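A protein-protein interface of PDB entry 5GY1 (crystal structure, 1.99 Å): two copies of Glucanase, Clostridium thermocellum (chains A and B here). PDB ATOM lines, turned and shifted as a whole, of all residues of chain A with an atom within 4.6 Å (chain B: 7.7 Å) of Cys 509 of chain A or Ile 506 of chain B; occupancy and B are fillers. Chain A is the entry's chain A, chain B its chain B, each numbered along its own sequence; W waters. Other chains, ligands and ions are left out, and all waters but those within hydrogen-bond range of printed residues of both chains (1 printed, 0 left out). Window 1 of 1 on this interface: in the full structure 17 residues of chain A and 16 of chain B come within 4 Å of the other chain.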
ATOM      1  N   ILE A 506     -14.427 -21.529 -21.185  1.00  0.00           N
ATOM      2  CA  ILE A 506     -14.854 -21.270 -19.819  1.00  0.00           C
ATOM      3  C   ILE A 506     -15.233 -19.802 -19.685  1.00  0.00           C
ATOM      4  O   ILE A 506     -14.468 -18.939 -20.092  1.00  0.00           O
ATOM      5  CB  ILE A 506     -13.700 -21.582 -18.840  1.00  0.00           C
ATOM      6  CG1 ILE A 506     -13.322 -23.059 -18.927  1.00  0.00           C
ATOM      7  CG2 ILE A 506     -14.080 -21.193 -17.412  1.00  0.00           C
ATOM      8  CD1 ILE A 506     -14.500 -24.001 -18.901  1.00  0.00           C
ATOM      9  N   TYR A 508     -16.490 -18.525 -16.550  1.00  0.00           N
ATOM     10  CA  TYR A 508     -16.355 -18.187 -15.137  1.00  0.00           C
ATOM     11  C   TYR A 508     -15.906 -19.458 -14.428  1.00  0.00           C
ATOM     12  O   TYR A 508     -16.487 -20.525 -14.635  1.00  0.00           O
ATOM     13  CB  TYR A 508     -17.685 -17.755 -14.488  1.00  0.00           C
ATOM     14  CG  TYR A 508     -17.583 -17.578 -12.981  1.00  0.00           C
ATOM     15  CD1 TYR A 508     -16.672 -16.684 -12.420  1.00  0.00           C
ATOM     16  CD2 TYR A 508     -18.408 -18.297 -12.108  1.00  0.00           C
ATOM     17  CE1 TYR A 508     -16.558 -16.527 -11.018  1.00  0.00           C
ATOM     18  CE2 TYR A 508     -18.311 -18.141 -10.718  1.00  0.00           C
ATOM     19  CZ  TYR A 508     -17.388 -17.259 -10.179  1.00  0.00           C
ATOM     20  OH  TYR A 508     -17.305 -17.096  -8.808  1.00  0.00           O
ATOM     21  N   CYS A 509     -14.885 -19.333 -13.590  1.00  0.00           N
ATOM     22  CA  CYS A 509     -14.543 -20.439 -12.716  1.00  0.00           C
ATOM     23  C   CYS A 509     -14.230 -19.861 -11.337  1.00  0.00           C
ATOM     24  O   CYS A 509     -13.453 -18.915 -11.186  1.00  0.00           O
ATOM     25  CB  CYS A 509     -13.466 -21.332 -13.341  1.00  0.00           C
ATOM     26  SG  CYS A 509     -11.808 -20.712 -13.275  1.00  0.00           S
ATOM     27  N   GLU A 510     -14.965 -20.358 -10.353  1.00  0.00           N
ATOM     28  CA  GLU A 510     -14.935 -19.819  -8.992  1.00  0.00           C
ATOM     29  C   GLU A 510     -13.550 -19.850  -8.349  1.00  0.00           C
ATOM     30  O   GLU A 510     -12.838 -20.867  -8.397  1.00  0.00           O
ATOM     31  CB  GLU A 510     -15.941 -20.593  -8.131  1.00  0.00           C
ATOM     32  CG  GLU A 510     -16.021 -20.101  -6.701  1.00  0.00           C
ATOM     33  CD  GLU A 510     -17.121 -20.773  -5.885  1.00  0.00           C
ATOM     34  OE1 GLU A 510     -17.978 -21.493  -6.449  1.00  0.00           O
ATOM     35  OE2 GLU A 510     -17.142 -20.532  -4.658  1.00  0.00           O
ATOM     36  N   SER A 511     -13.192 -18.732  -7.723  1.00  0.00           N
ATOM     37  CA  SER A 511     -11.913 -18.603  -7.052  1.00  0.00           C
ATOM     38  C   SER A 511     -11.669 -19.727  -6.044  1.00  0.00           C
ATOM     39  O   SER A 511     -12.562 -20.077  -5.271  1.00  0.00           O
ATOM     40  CB  SER A 511     -11.842 -17.246  -6.353  1.00  0.00           C
ATOM     41  OG  SER A 511     -10.554 -17.096  -5.801  1.00  0.00           O
ATOM     42  N   MET A 513     -11.087 -22.921  -6.486  1.00  0.00           N
ATOM     43  CA  MET A 513     -11.552 -24.251  -6.888  1.00  0.00           C
ATOM     44  C   MET A 513     -10.774 -24.772  -8.106  1.00  0.00           C
ATOM     45  O   MET A 513     -11.257 -24.692  -9.240  1.00  0.00           O
ATOM     46  CB  MET A 513     -13.051 -24.224  -7.203  1.00  0.00           C
ATOM     47  CG  MET A 513     -13.975 -23.689  -6.114  1.00  0.00           C
ATOM     48  SD  MET A 513     -13.864 -24.640  -4.576  1.00  0.00           S
ATOM     49  CE  MET A 513     -15.430 -24.118  -3.851  1.00  0.00           C
ATOM     50  N   ASP A 514      -9.588 -25.324  -7.865  1.00  0.00           N
ATOM     51  CA  ASP A 514      -8.681 -25.771  -8.925  1.00  0.00           C
ATOM     52  C   ASP A 514      -9.397 -26.799  -9.793  1.00  0.00           C
ATOM     53  O   ASP A 514      -9.801 -27.850  -9.296  1.00  0.00           O
ATOM     54  CB  ASP A 514      -7.457 -26.403  -8.261  1.00  0.00           C
ATOM     55  CG  ASP A 514      -6.310 -26.689  -9.222  1.00  0.00           C
ATOM     56  OD1 ASP A 514      -6.128 -25.954 -10.224  1.00  0.00           O
ATOM     57  OD2 ASP A 514      -5.557 -27.657  -8.940  1.00  0.00           O
ATOM     58  N   VAL A 515      -9.570 -26.491 -11.074  1.00  0.00           N
ATOM     59  CA  VAL A 515     -10.413 -27.321 -11.926  1.00  0.00           C
ATOM     60  C   VAL A 515      -9.728 -27.659 -13.253  1.00  0.00           C
ATOM     61  O   VAL A 515      -8.929 -26.875 -13.783  1.00  0.00           O
ATOM     62  CB  VAL A 515     -11.810 -26.687 -12.127  1.00  0.00           C
ATOM     63  CG1 VAL A 515     -11.735 -25.361 -12.877  1.00  0.00           C
ATOM     64  CG2 VAL A 515     -12.772 -27.641 -12.831  1.00  0.00           C
ATOM     65  N   ILE A 517     -10.811 -29.363 -17.237  1.00  0.00           N
ATOM     66  CA  ILE A 517     -11.876 -29.826 -18.119  1.00  0.00           C
ATOM     67  C   ILE A 517     -11.188 -30.654 -19.192  1.00  0.00           C
ATOM     68  O   ILE A 517     -10.200 -30.204 -19.767  1.00  0.00           O
ATOM     69  CB  ILE A 517     -12.688 -28.669 -18.744  1.00  0.00           C
ATOM     70  CG1 ILE A 517     -13.354 -27.820 -17.655  1.00  0.00           C
ATOM     71  CG2 ILE A 517     -13.821 -29.241 -19.598  1.00  0.00           C
ATOM     72  CD1 ILE A 517     -12.490 -26.734 -17.048  1.00  0.00           C
ATOM     73  N   GLU A 551     -18.788 -23.313  -8.585  1.00  0.00           N
ATOM     74  CA  GLU A 551     -19.474 -22.859  -9.770  1.00  0.00           C
ATOM     75  C   GLU A 551     -18.503 -22.783 -10.942  1.00  0.00           C
ATOM     76  O   GLU A 551     -17.424 -22.200 -10.820  1.00  0.00           O
ATOM     77  CB  GLU A 551     -20.125 -21.489  -9.539  1.00  0.00           C
ATOM     78  CG  GLU A 551     -20.728 -20.957 -10.836  1.00  0.00           C
ATOM     79  CD  GLU A 551     -21.629 -19.746 -10.639  1.00  0.00           C
ATOM     80  OE1 GLU A 551     -21.914 -19.389  -9.483  1.00  0.00           O
ATOM     81  OE2 GLU A 551     -22.085 -19.166 -11.645  1.00  0.00           O
ATOM     82  N   LEU A 552     -18.937 -23.330 -12.078  1.00  0.00           N
ATOM     83  CA  LEU A 552     -18.200 -23.243 -13.333  1.00  0.00           C
ATOM     84  C   LEU A 552     -19.207 -22.913 -14.419  1.00  0.00           C
ATOM     85  O   LEU A 552     -20.295 -23.489 -14.443  1.00  0.00           O
ATOM     86  CB  LEU A 552     -17.513 -24.583 -13.637  1.00  0.00           C
ATOM     87  CG  LEU A 552     -16.757 -24.760 -14.956  1.00  0.00           C
ATOM     88  CD1 LEU A 552     -15.517 -23.880 -14.925  1.00  0.00           C
ATOM     89  CD2 LEU A 552     -16.374 -26.239 -15.249  1.00  0.00           C
ATOM     90  N   GLU B 462       1.910 -21.997  -9.745  1.00  0.00           N
ATOM     91  CA  GLU B 462       0.614 -21.366  -9.944  1.00  0.00           C
ATOM     92  C   GLU B 462       0.789 -19.878 -10.186  1.00  0.00           C
ATOM     93  O   GLU B 462       1.375 -19.186  -9.347  1.00  0.00           O
ATOM     94  CB  GLU B 462      -0.325 -21.598  -8.761  1.00  0.00           C
ATOM     95  CG  GLU B 462      -1.744 -21.120  -9.050  1.00  0.00           C
ATOM     96  CD  GLU B 462      -2.713 -21.541  -7.959  1.00  0.00           C
ATOM     97  OE1 GLU B 462      -3.161 -22.708  -7.960  1.00  0.00           O
ATOM     98  OE2 GLU B 462      -3.002 -20.700  -7.087  1.00  0.00           O
ATOM     99  N   LYS B 503       0.053 -31.427 -15.802  1.00  0.00           N
ATOM    100  CA  LYS B 503      -1.373 -31.117 -15.838  1.00  0.00           C
ATOM    101  C   LYS B 503      -1.576 -29.603 -15.730  1.00  0.00           C
ATOM    102  O   LYS B 503      -0.985 -28.958 -14.858  1.00  0.00           O
ATOM    103  CB  LYS B 503      -2.045 -31.802 -14.644  1.00  0.00           C
ATOM    104  CG  LYS B 503      -3.568 -31.867 -14.711  1.00  0.00           C
ATOM    105  CD  LYS B 503      -4.197 -32.249 -13.371  1.00  0.00           C
ATOM    106  CE  LYS B 503      -3.826 -33.658 -12.925  1.00  0.00           C
ATOM    107  NZ  LYS B 503      -4.604 -34.660 -13.694  1.00  0.00           N
ATOM    108  N   VAL B 504      -2.424 -29.054 -16.595  1.00  0.00           N
ATOM    109  CA  VAL B 504      -2.788 -27.633 -16.548  1.00  0.00           C
ATOM    110  C   VAL B 504      -4.197 -27.465 -15.963  1.00  0.00           C
ATOM    111  O   VAL B 504      -5.140 -28.055 -16.478  1.00  0.00           O
ATOM    112  CB  VAL B 504      -2.740 -27.014 -17.960  1.00  0.00           C
ATOM    113  CG1 VAL B 504      -3.083 -25.524 -17.889  1.00  0.00           C
ATOM    114  CG2 VAL B 504      -1.348 -27.203 -18.556  1.00  0.00           C
ATOM    115  N   THR B 505      -4.336 -26.662 -14.911  1.00  0.00           N
ATOM    116  CA  THR B 505      -5.632 -26.467 -14.253  1.00  0.00           C
ATOM    117  C   THR B 505      -5.884 -24.970 -14.056  1.00  0.00           C
ATOM    118  O   THR B 505      -4.961 -24.169 -14.237  1.00  0.00           O
ATOM    119  CB  THR B 505      -5.738 -27.222 -12.915  1.00  0.00           C
ATOM    120  OG1 THR B 505      -4.622 -26.889 -12.075  1.00  0.00           O
ATOM    121  CG2 THR B 505      -5.761 -28.733 -13.140  1.00  0.00           C
ATOM    122  N   ILE B 506      -7.121 -24.593 -13.737  1.00  0.00           N
ATOM    123  CA  ILE B 506      -7.460 -23.188 -13.531  1.00  0.00           C
ATOM    124  C   ILE B 506      -8.060 -23.027 -12.135  1.00  0.00           C
ATOM    125  O   ILE B 506      -8.886 -23.836 -11.710  1.00  0.00           O
ATOM    126  CB  ILE B 506      -8.402 -22.616 -14.623  1.00  0.00           C
ATOM    127  CG1 ILE B 506      -9.688 -23.436 -14.730  1.00  0.00           C
ATOM    128  CG2 ILE B 506      -7.717 -22.574 -15.997  1.00  0.00           C
ATOM    129  CD1 ILE B 506     -10.441 -23.279 -16.050  1.00  0.00           C
ATOM    130  N   GLY B 507      -7.586 -22.015 -11.416  1.00  0.00           N
ATOM    131  CA  GLY B 507      -7.978 -21.781 -10.033  1.00  0.00           C
ATOM    132  C   GLY B 507      -8.894 -20.580  -9.865  1.00  0.00           C
ATOM    133  O   GLY B 507      -9.445 -20.384  -8.776  1.00  0.00           O
ATOM    134  N   TYR B 508      -9.064 -19.796 -10.933  1.00  0.00           N
ATOM    135  CA  TYR B 508      -9.969 -18.631 -10.979  1.00  0.00           C
ATOM    136  C   TYR B 508      -9.968 -18.127 -12.420  1.00  0.00           C
ATOM    137  O   TYR B 508      -8.892 -17.969 -12.990  1.00  0.00           O
ATOM    138  CB  TYR B 508      -9.521 -17.478 -10.065  1.00  0.00           C
ATOM    139  CG  TYR B 508     -10.347 -16.222 -10.252  1.00  0.00           C
ATOM    140  CD1 TYR B 508     -11.720 -16.218 -10.002  1.00  0.00           C
ATOM    141  CD2 TYR B 508      -9.767 -15.053 -10.730  1.00  0.00           C
ATOM    142  CE1 TYR B 508     -12.483 -15.080 -10.201  1.00  0.00           C
ATOM    143  CE2 TYR B 508     -10.517 -13.898 -10.924  1.00  0.00           C
ATOM    144  CZ  TYR B 508     -11.865 -13.918 -10.652  1.00  0.00           C
ATOM    145  OH  TYR B 508     -12.597 -12.779 -10.877  1.00  0.00           O
ATOM    146  N   CYS B 509     -11.159 -17.902 -12.979  1.00  0.00           N
ATOM    147  CA  CYS B 509     -11.360 -17.325 -14.312  1.00  0.00           C
ATOM    148  C   CYS B 509     -12.420 -16.252 -14.146  1.00  0.00           C
ATOM    149  O   CYS B 509     -13.568 -16.560 -13.824  1.00  0.00           O
ATOM    150  CB  CYS B 509     -11.923 -18.347 -15.314  1.00  0.00           C
ATOM    151  SG  CYS B 509     -11.258 -20.015 -15.137  1.00  0.00           S
ATOM    152  N   GLU B 510     -12.049 -15.006 -14.406  1.00  0.00           N
ATOM    153  CA  GLU B 510     -12.964 -13.892 -14.186  1.00  0.00           C
ATOM    154  C   GLU B 510     -14.268 -14.010 -14.981  1.00  0.00           C
ATOM    155  O   GLU B 510     -14.251 -14.302 -16.176  1.00  0.00           O
ATOM    156  CB  GLU B 510     -12.247 -12.591 -14.532  1.00  0.00           C
ATOM    157  CG  GLU B 510     -13.137 -11.365 -14.415  1.00  0.00           C
ATOM    158  CD  GLU B 510     -12.404 -10.084 -14.789  1.00  0.00           C
ATOM    159  OE1 GLU B 510     -11.163 -10.124 -14.936  1.00  0.00           O
ATOM    160  OE2 GLU B 510     -13.066  -9.028 -14.879  1.00  0.00           O
ATOM    161  N   SER B 511     -15.397 -13.779 -14.316  1.00  0.00           N
ATOM    162  CA  SER B 511     -16.721 -13.880 -14.943  1.00  0.00           C
ATOM    163  C   SER B 511     -16.857 -13.010 -16.199  1.00  0.00           C
ATOM    164  O   SER B 511     -16.490 -11.838 -16.173  1.00  0.00           O
ATOM    165  CB  SER B 511     -17.783 -13.441 -13.922  1.00  0.00           C
ATOM    166  OG  SER B 511     -19.070 -13.623 -14.475  1.00  0.00           O
ATOM    167  N   GLY B 512     -17.384 -13.556 -17.288  1.00  0.00           N
ATOM    168  CA  GLY B 512     -17.587 -12.769 -18.503  1.00  0.00           C
ATOM    169  C   GLY B 512     -16.430 -12.708 -19.491  1.00  0.00           C
ATOM    170  O   GLY B 512     -16.573 -12.140 -20.579  1.00  0.00           O
ATOM    171  N   VAL B 515     -12.698 -17.854 -22.118  1.00  0.00           N
ATOM    172  CA  VAL B 515     -11.278 -18.172 -22.203  1.00  0.00           C
ATOM    173  C   VAL B 515     -11.068 -19.648 -22.591  1.00  0.00           C
ATOM    174  O   VAL B 515     -11.862 -20.546 -22.241  1.00  0.00           O
ATOM    175  CB  VAL B 515     -10.549 -17.780 -20.874  1.00  0.00           C
ATOM    176  CG1 VAL B 515     -10.842 -18.783 -19.764  1.00  0.00           C
ATOM    177  CG2 VAL B 515      -9.029 -17.692 -21.071  1.00  0.00           C
ATOM    178  N   GLU B 516      -9.997 -19.873 -23.345  1.00  0.00           N
ATOM    179  CA  GLU B 516      -9.506 -21.219 -23.596  1.00  0.00           C
ATOM    180  C   GLU B 516      -8.010 -21.280 -23.318  1.00  0.00           C
ATOM    181  O   GLU B 516      -7.306 -20.281 -23.471  1.00  0.00           O
ATOM    182  CB  GLU B 516      -9.807 -21.655 -25.031  1.00  0.00           C
ATOM    183  CG  GLU B 516      -8.888 -21.104 -26.108  1.00  0.00           C
ATOM    184  CD  GLU B 516      -9.506 -21.179 -27.505  1.00  0.00           C
ATOM    185  OE1 GLU B 516     -10.539 -21.863 -27.672  1.00  0.00           O
ATOM    186  OE2 GLU B 516      -8.965 -20.548 -28.441  1.00  0.00           O
ATOM    187  N   ILE B 517      -7.537 -22.454 -22.900  1.00  0.00           N
ATOM    188  CA  ILE B 517      -6.117 -22.660 -22.666  1.00  0.00           C
ATOM    189  C   ILE B 517      -5.683 -23.839 -23.521  1.00  0.00           C
ATOM    190  O   ILE B 517      -6.296 -24.913 -23.491  1.00  0.00           O
ATOM    191  CB  ILE B 517      -5.826 -22.897 -21.166  1.00  0.00           C
ATOM    192  CG1 ILE B 517      -6.311 -21.690 -20.360  1.00  0.00           C
ATOM    193  CG2 ILE B 517      -4.327 -23.061 -20.901  1.00  0.00           C
ATOM    194  CD1 ILE B 517      -5.961 -21.779 -18.878  1.00  0.00           C
ATOM    195  N   ILE B 532      -3.001 -18.910 -23.634  1.00  0.00           N
ATOM    196  CA  ILE B 532      -4.273 -18.519 -23.062  1.00  0.00           C
ATOM    197  C   ILE B 532      -4.922 -17.593 -24.089  1.00  0.00           C
ATOM    198  O   ILE B 532      -4.343 -16.555 -24.405  1.00  0.00           O
ATOM    199  CB  ILE B 532      -4.052 -17.726 -21.749  1.00  0.00           C
ATOM    200  CG1 ILE B 532      -3.507 -18.621 -20.626  1.00  0.00           C
ATOM    201  CG2 ILE B 532      -5.368 -17.110 -21.286  1.00  0.00           C
ATOM    202  CD1 ILE B 532      -2.055 -19.082 -20.774  1.00  0.00           C
ATOM    203  N   GLU B 551      -8.494 -11.407 -15.469  1.00  0.00           N
ATOM    204  CA  GLU B 551      -7.687 -12.148 -14.509  1.00  0.00           C
ATOM    205  C   GLU B 551      -7.926 -13.648 -14.655  1.00  0.00           C
ATOM    206  O   GLU B 551      -9.070 -14.095 -14.708  1.00  0.00           O
ATOM    207  CB  GLU B 551      -7.984 -11.736 -13.064  1.00  0.00           C
ATOM    208  CG  GLU B 551      -7.263 -12.630 -12.059  1.00  0.00           C
ATOM    209  CD  GLU B 551      -7.320 -12.078 -10.647  1.00  0.00           C
ATOM    210  OE1 GLU B 551      -7.774 -10.929 -10.497  1.00  0.00           O
ATOM    211  OE2 GLU B 551      -6.947 -12.800  -9.700  1.00  0.00           O
ATOM    212  N   LEU B 552      -6.834 -14.404 -14.702  1.00  0.00           N
ATOM    213  CA  LEU B 552      -6.880 -15.857 -14.743  1.00  0.00           C
ATOM    214  C   LEU B 552      -5.855 -16.382 -13.729  1.00  0.00           C
ATOM    215  O   LEU B 552      -4.731 -15.874 -13.664  1.00  0.00           O
ATOM    216  CB  LEU B 552      -6.517 -16.324 -16.151  1.00  0.00           C
ATOM    217  CG  LEU B 552      -6.438 -17.844 -16.344  1.00  0.00           C
ATOM    218  CD1 LEU B 552      -7.823 -18.452 -16.263  1.00  0.00           C
ATOM    219  CD2 LEU B 552      -5.769 -18.174 -17.671  1.00  0.00           C
ATOM    220  N   GLN B 553      -6.228 -17.357 -12.903  1.00  0.00           N
ATOM    221  CA  GLN B 553      -5.196 -18.074 -12.156  1.00  0.00           C
ATOM    222  C   GLN B 553      -5.032 -19.458 -12.767  1.00  0.00           C
ATOM    223  O   GLN B 553      -5.998 -20.214 -12.853  1.00  0.00           O
ATOM    224  CB  GLN B 553      -5.528 -18.167 -10.661  1.00  0.00           C
ATOM    225  CG  GLN B 553      -5.503 -16.805  -9.973  1.00  0.00           C
ATOM    226  CD  GLN B 553      -5.999 -16.835  -8.533  1.00  0.00           C
ATOM    227  OE1 GLN B 553      -5.832 -17.829  -7.825  1.00  0.00           O
ATOM    228  NE2 GLN B 553      -6.623 -15.741  -8.101  1.00  0.00           N
ATOM    229  N   PHE B 554      -3.829 -19.784 -13.230  1.00  0.00           N
ATOM    230  CA  PHE B 554      -3.605 -21.112 -13.784  1.00  0.00           C
ATOM    231  C   PHE B 554      -2.477 -21.828 -13.048  1.00  0.00           C
ATOM    232  O   PHE B 554      -1.534 -21.217 -12.539  1.00  0.00           O
ATOM    233  CB  PHE B 554      -3.371 -21.112 -15.300  1.00  0.00           C
ATOM    234  CG  PHE B 554      -2.186 -20.287 -15.754  1.00  0.00           C
ATOM    235  CD1 PHE B 554      -2.329 -18.929 -16.016  1.00  0.00           C
ATOM    236  CD2 PHE B 554      -0.939 -20.877 -15.942  1.00  0.00           C
ATOM    237  CE1 PHE B 554      -1.238 -18.169 -16.441  1.00  0.00           C
ATOM    238  CE2 PHE B 554       0.148 -20.137 -16.396  1.00  0.00           C
ATOM    239  CZ  PHE B 554      -0.005 -18.779 -16.651  1.00  0.00           C
ATOM    240  N   ARG B 555      -2.594 -23.143 -13.015  1.00  0.00           N
ATOM    241  CA  ARG B 555      -1.592 -23.965 -12.371  1.00  0.00           C
ATOM    242  C   ARG B 555      -1.024 -24.978 -13.358  1.00  0.00           C
ATOM    243  O   ARG B 555      -1.766 -25.600 -14.119  1.00  0.00           O
ATOM    244  CB  ARG B 555      -2.175 -24.645 -11.128  1.00  0.00           C
ATOM    245  CG  ARG B 555      -1.194 -25.617 -10.479  1.00  0.00           C
ATOM    246  CD  ARG B 555      -1.881 -26.455  -9.402  1.00  0.00           C
ATOM    247  NE  ARG B 555      -2.345 -25.595  -8.316  1.00  0.00           N
ATOM    248  CZ  ARG B 555      -2.707 -26.039  -7.116  1.00  0.00           C
ATOM    249  NH1 ARG B 555      -2.657 -27.338  -6.844  1.00  0.00           N
ATOM    250  NH2 ARG B 555      -3.122 -25.181  -6.193  1.00  0.00           N
ATOM    251  N   ILE B 556       0.296 -25.133 -13.334  1.00  0.00           N
ATOM    252  CA  ILE B 556       0.962 -26.157 -14.136  1.00  0.00           C
ATOM    253  C   ILE B 556       1.696 -27.098 -13.186  1.00  0.00           C
ATOM    254  O   ILE B 556       2.596 -26.658 -12.460  1.00  0.00           O
ATOM    255  CB  ILE B 556       1.953 -25.530 -15.131  1.00  0.00           C
ATOM    256  CG1 ILE B 556       1.253 -24.413 -15.914  1.00  0.00           C
ATOM    257  CG2 ILE B 556       2.531 -26.611 -16.062  1.00  0.00           C
ATOM    258  CD1 ILE B 556       2.147 -23.685 -16.909  1.00  0.00           C
HETATM  259  O   HOH W   1      -5.406 -28.239  -6.340  1.00  0.00           O
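Ile 506 of chain A touches Cys 509 of chain B (CG2 to SG, 3.8 Å).
Tyr 508 of chain A touches Cys 509 of chain B.
Tyr 508 of chain A touches Ser 511 of chain B.
Ile 506 of chain B touches Cys 509 of chain A (CG1 to SG, 3.7 Å).
CA of Ser 511 of chain A touches O of Gly 507 of chain B (3.5 Å).
CD1 of Tyr 508 of chain B touches N of Ser 511 of chain A, 3.7 Å away.
Met 513 of chain A touches Ile 506 of chain B.
O of Gly 507 of chain B touches N of Met 513 of chain A, 3.8 Å away.
Asp 514 of chain A touches Ile 506 of chain B (CA to O, 3.4 Å).
Val 515 of chain A touches Thr 505 of chain B (O to CB, 3.3 Å).
The side-chain carboxylate (OE1) of Glu 510 of chain A sits at hydrogen-bond distance from the backbone NH (N) of Glu 551 of chain A.
OE1 of Glu 462 of chain B lies within salt-bridge range of NE of Arg 555 of chain B.
N of Arg 555 of chain B lies within hydrogen-bond range of O of Thr 505 of chain B, 2.9 Å away.
The backbone carbonyl oxygen of Gln 553 of chain B lies within hydrogen-bond range of the backbone NH of Gly 507 of chain B (2.8 Å).
N of Gln 553 of chain B is in hydrogen-bond range of O of Tyr 508 of chain B, 2.7 Å away.
The backbone NH (N) of Val 515 of chain B is in hydrogen-bond range of the backbone carbonyl oxygen (O) of Ile 506 of chain A (2.9 Å).
O of Gly 507 of chain B lies close to O of Glu 510 of chain A (3.4 Å).
The side-chain carboxylate (OD2) of Asp 514 of chain A is in salt-bridge range of the guanidinium group (NH1) of Arg 555 of chain B (3.6 Å).
SG of Cys 509 of chain A lies close to N of Tyr 508 of chain B, 3.7 Å away.
The side-chain carboxylate (OD1) of Asp 514 of chain A is in hydrogen-bond range of the side-chain hydroxyl (OG1) of Thr 505 of chain B, 2.6 Å away.
N of Val 515 of chain A lies within hydrogen-bond range of O of Ile 506 of chain B, at 2.8 Å.
SG of Cys 509 of chain A is disulfide-bonded to SG of Cys 509 of chain B, at 2.1 Å.
Of the printed residues of chain B, Tyr 508 of chain A touches Cys 509 (3.4 Å) and Ser 511 (3.7 Å).
Of chain B, only Ile 506, Tyr 508 and Cys 509 come within 4 Å of Cys 509 of chain A.
Printed residues of chain B within 4 Å of Ser 511 of chain A: Gly 507 and Tyr 508.
Printed residues of chain A within 4 Å of Thr 505 of chain B: Asp 514 (2.6 Å) and Val 515 (3.3 Å).
Of chain A, only Cys 509 (3.7 Å), Met 513 (3.5 Å), Asp 514 (3.4 Å) and Val 515 (2.8 Å) come within 4 Å of Ile 506 of chain B.
Printed residues of chain A within 4 Å of Tyr 508 of chain B: Cys 509 and Ser 511.
The nearest residue of chain B that does not touch Cys 509 of chain A is Gly 507 of chain B (4.5 Å).
Ile 506 of chain A touches Cys 509 of chain B, and with the chains exchanged Cys 509 of chain A touches Ile 506 of chain B.
Ile 506 of chain A touches Val 515 of chain B, and with the chains exchanged Val 515 of chain A touches Ile 506 of chain B.
Tyr 508 of chain A touches Cys 509 of chain B, and with the chains exchanged Cys 509 of chain A touches Tyr 508 of chain B.
Cys 509 of chain A touches its own counterpart, Cys 509 of chain B.
Water W1 bridges the side-chain carboxylate (OD2) of Asp 514 of chain A (2.7 Å) and the guanidinium group (NH1) of Arg 555 of chain B (2.9 Å).
Of the 11 printed residues of chain A, 8 touch a printed residue of chain B.
Among the printed residues, Asp or Glu carboxylates within 4 Å of a Lys or Arg side-chain nitrogen of the other chain: Asp 514 of chain A with Arg 555 of chain B.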
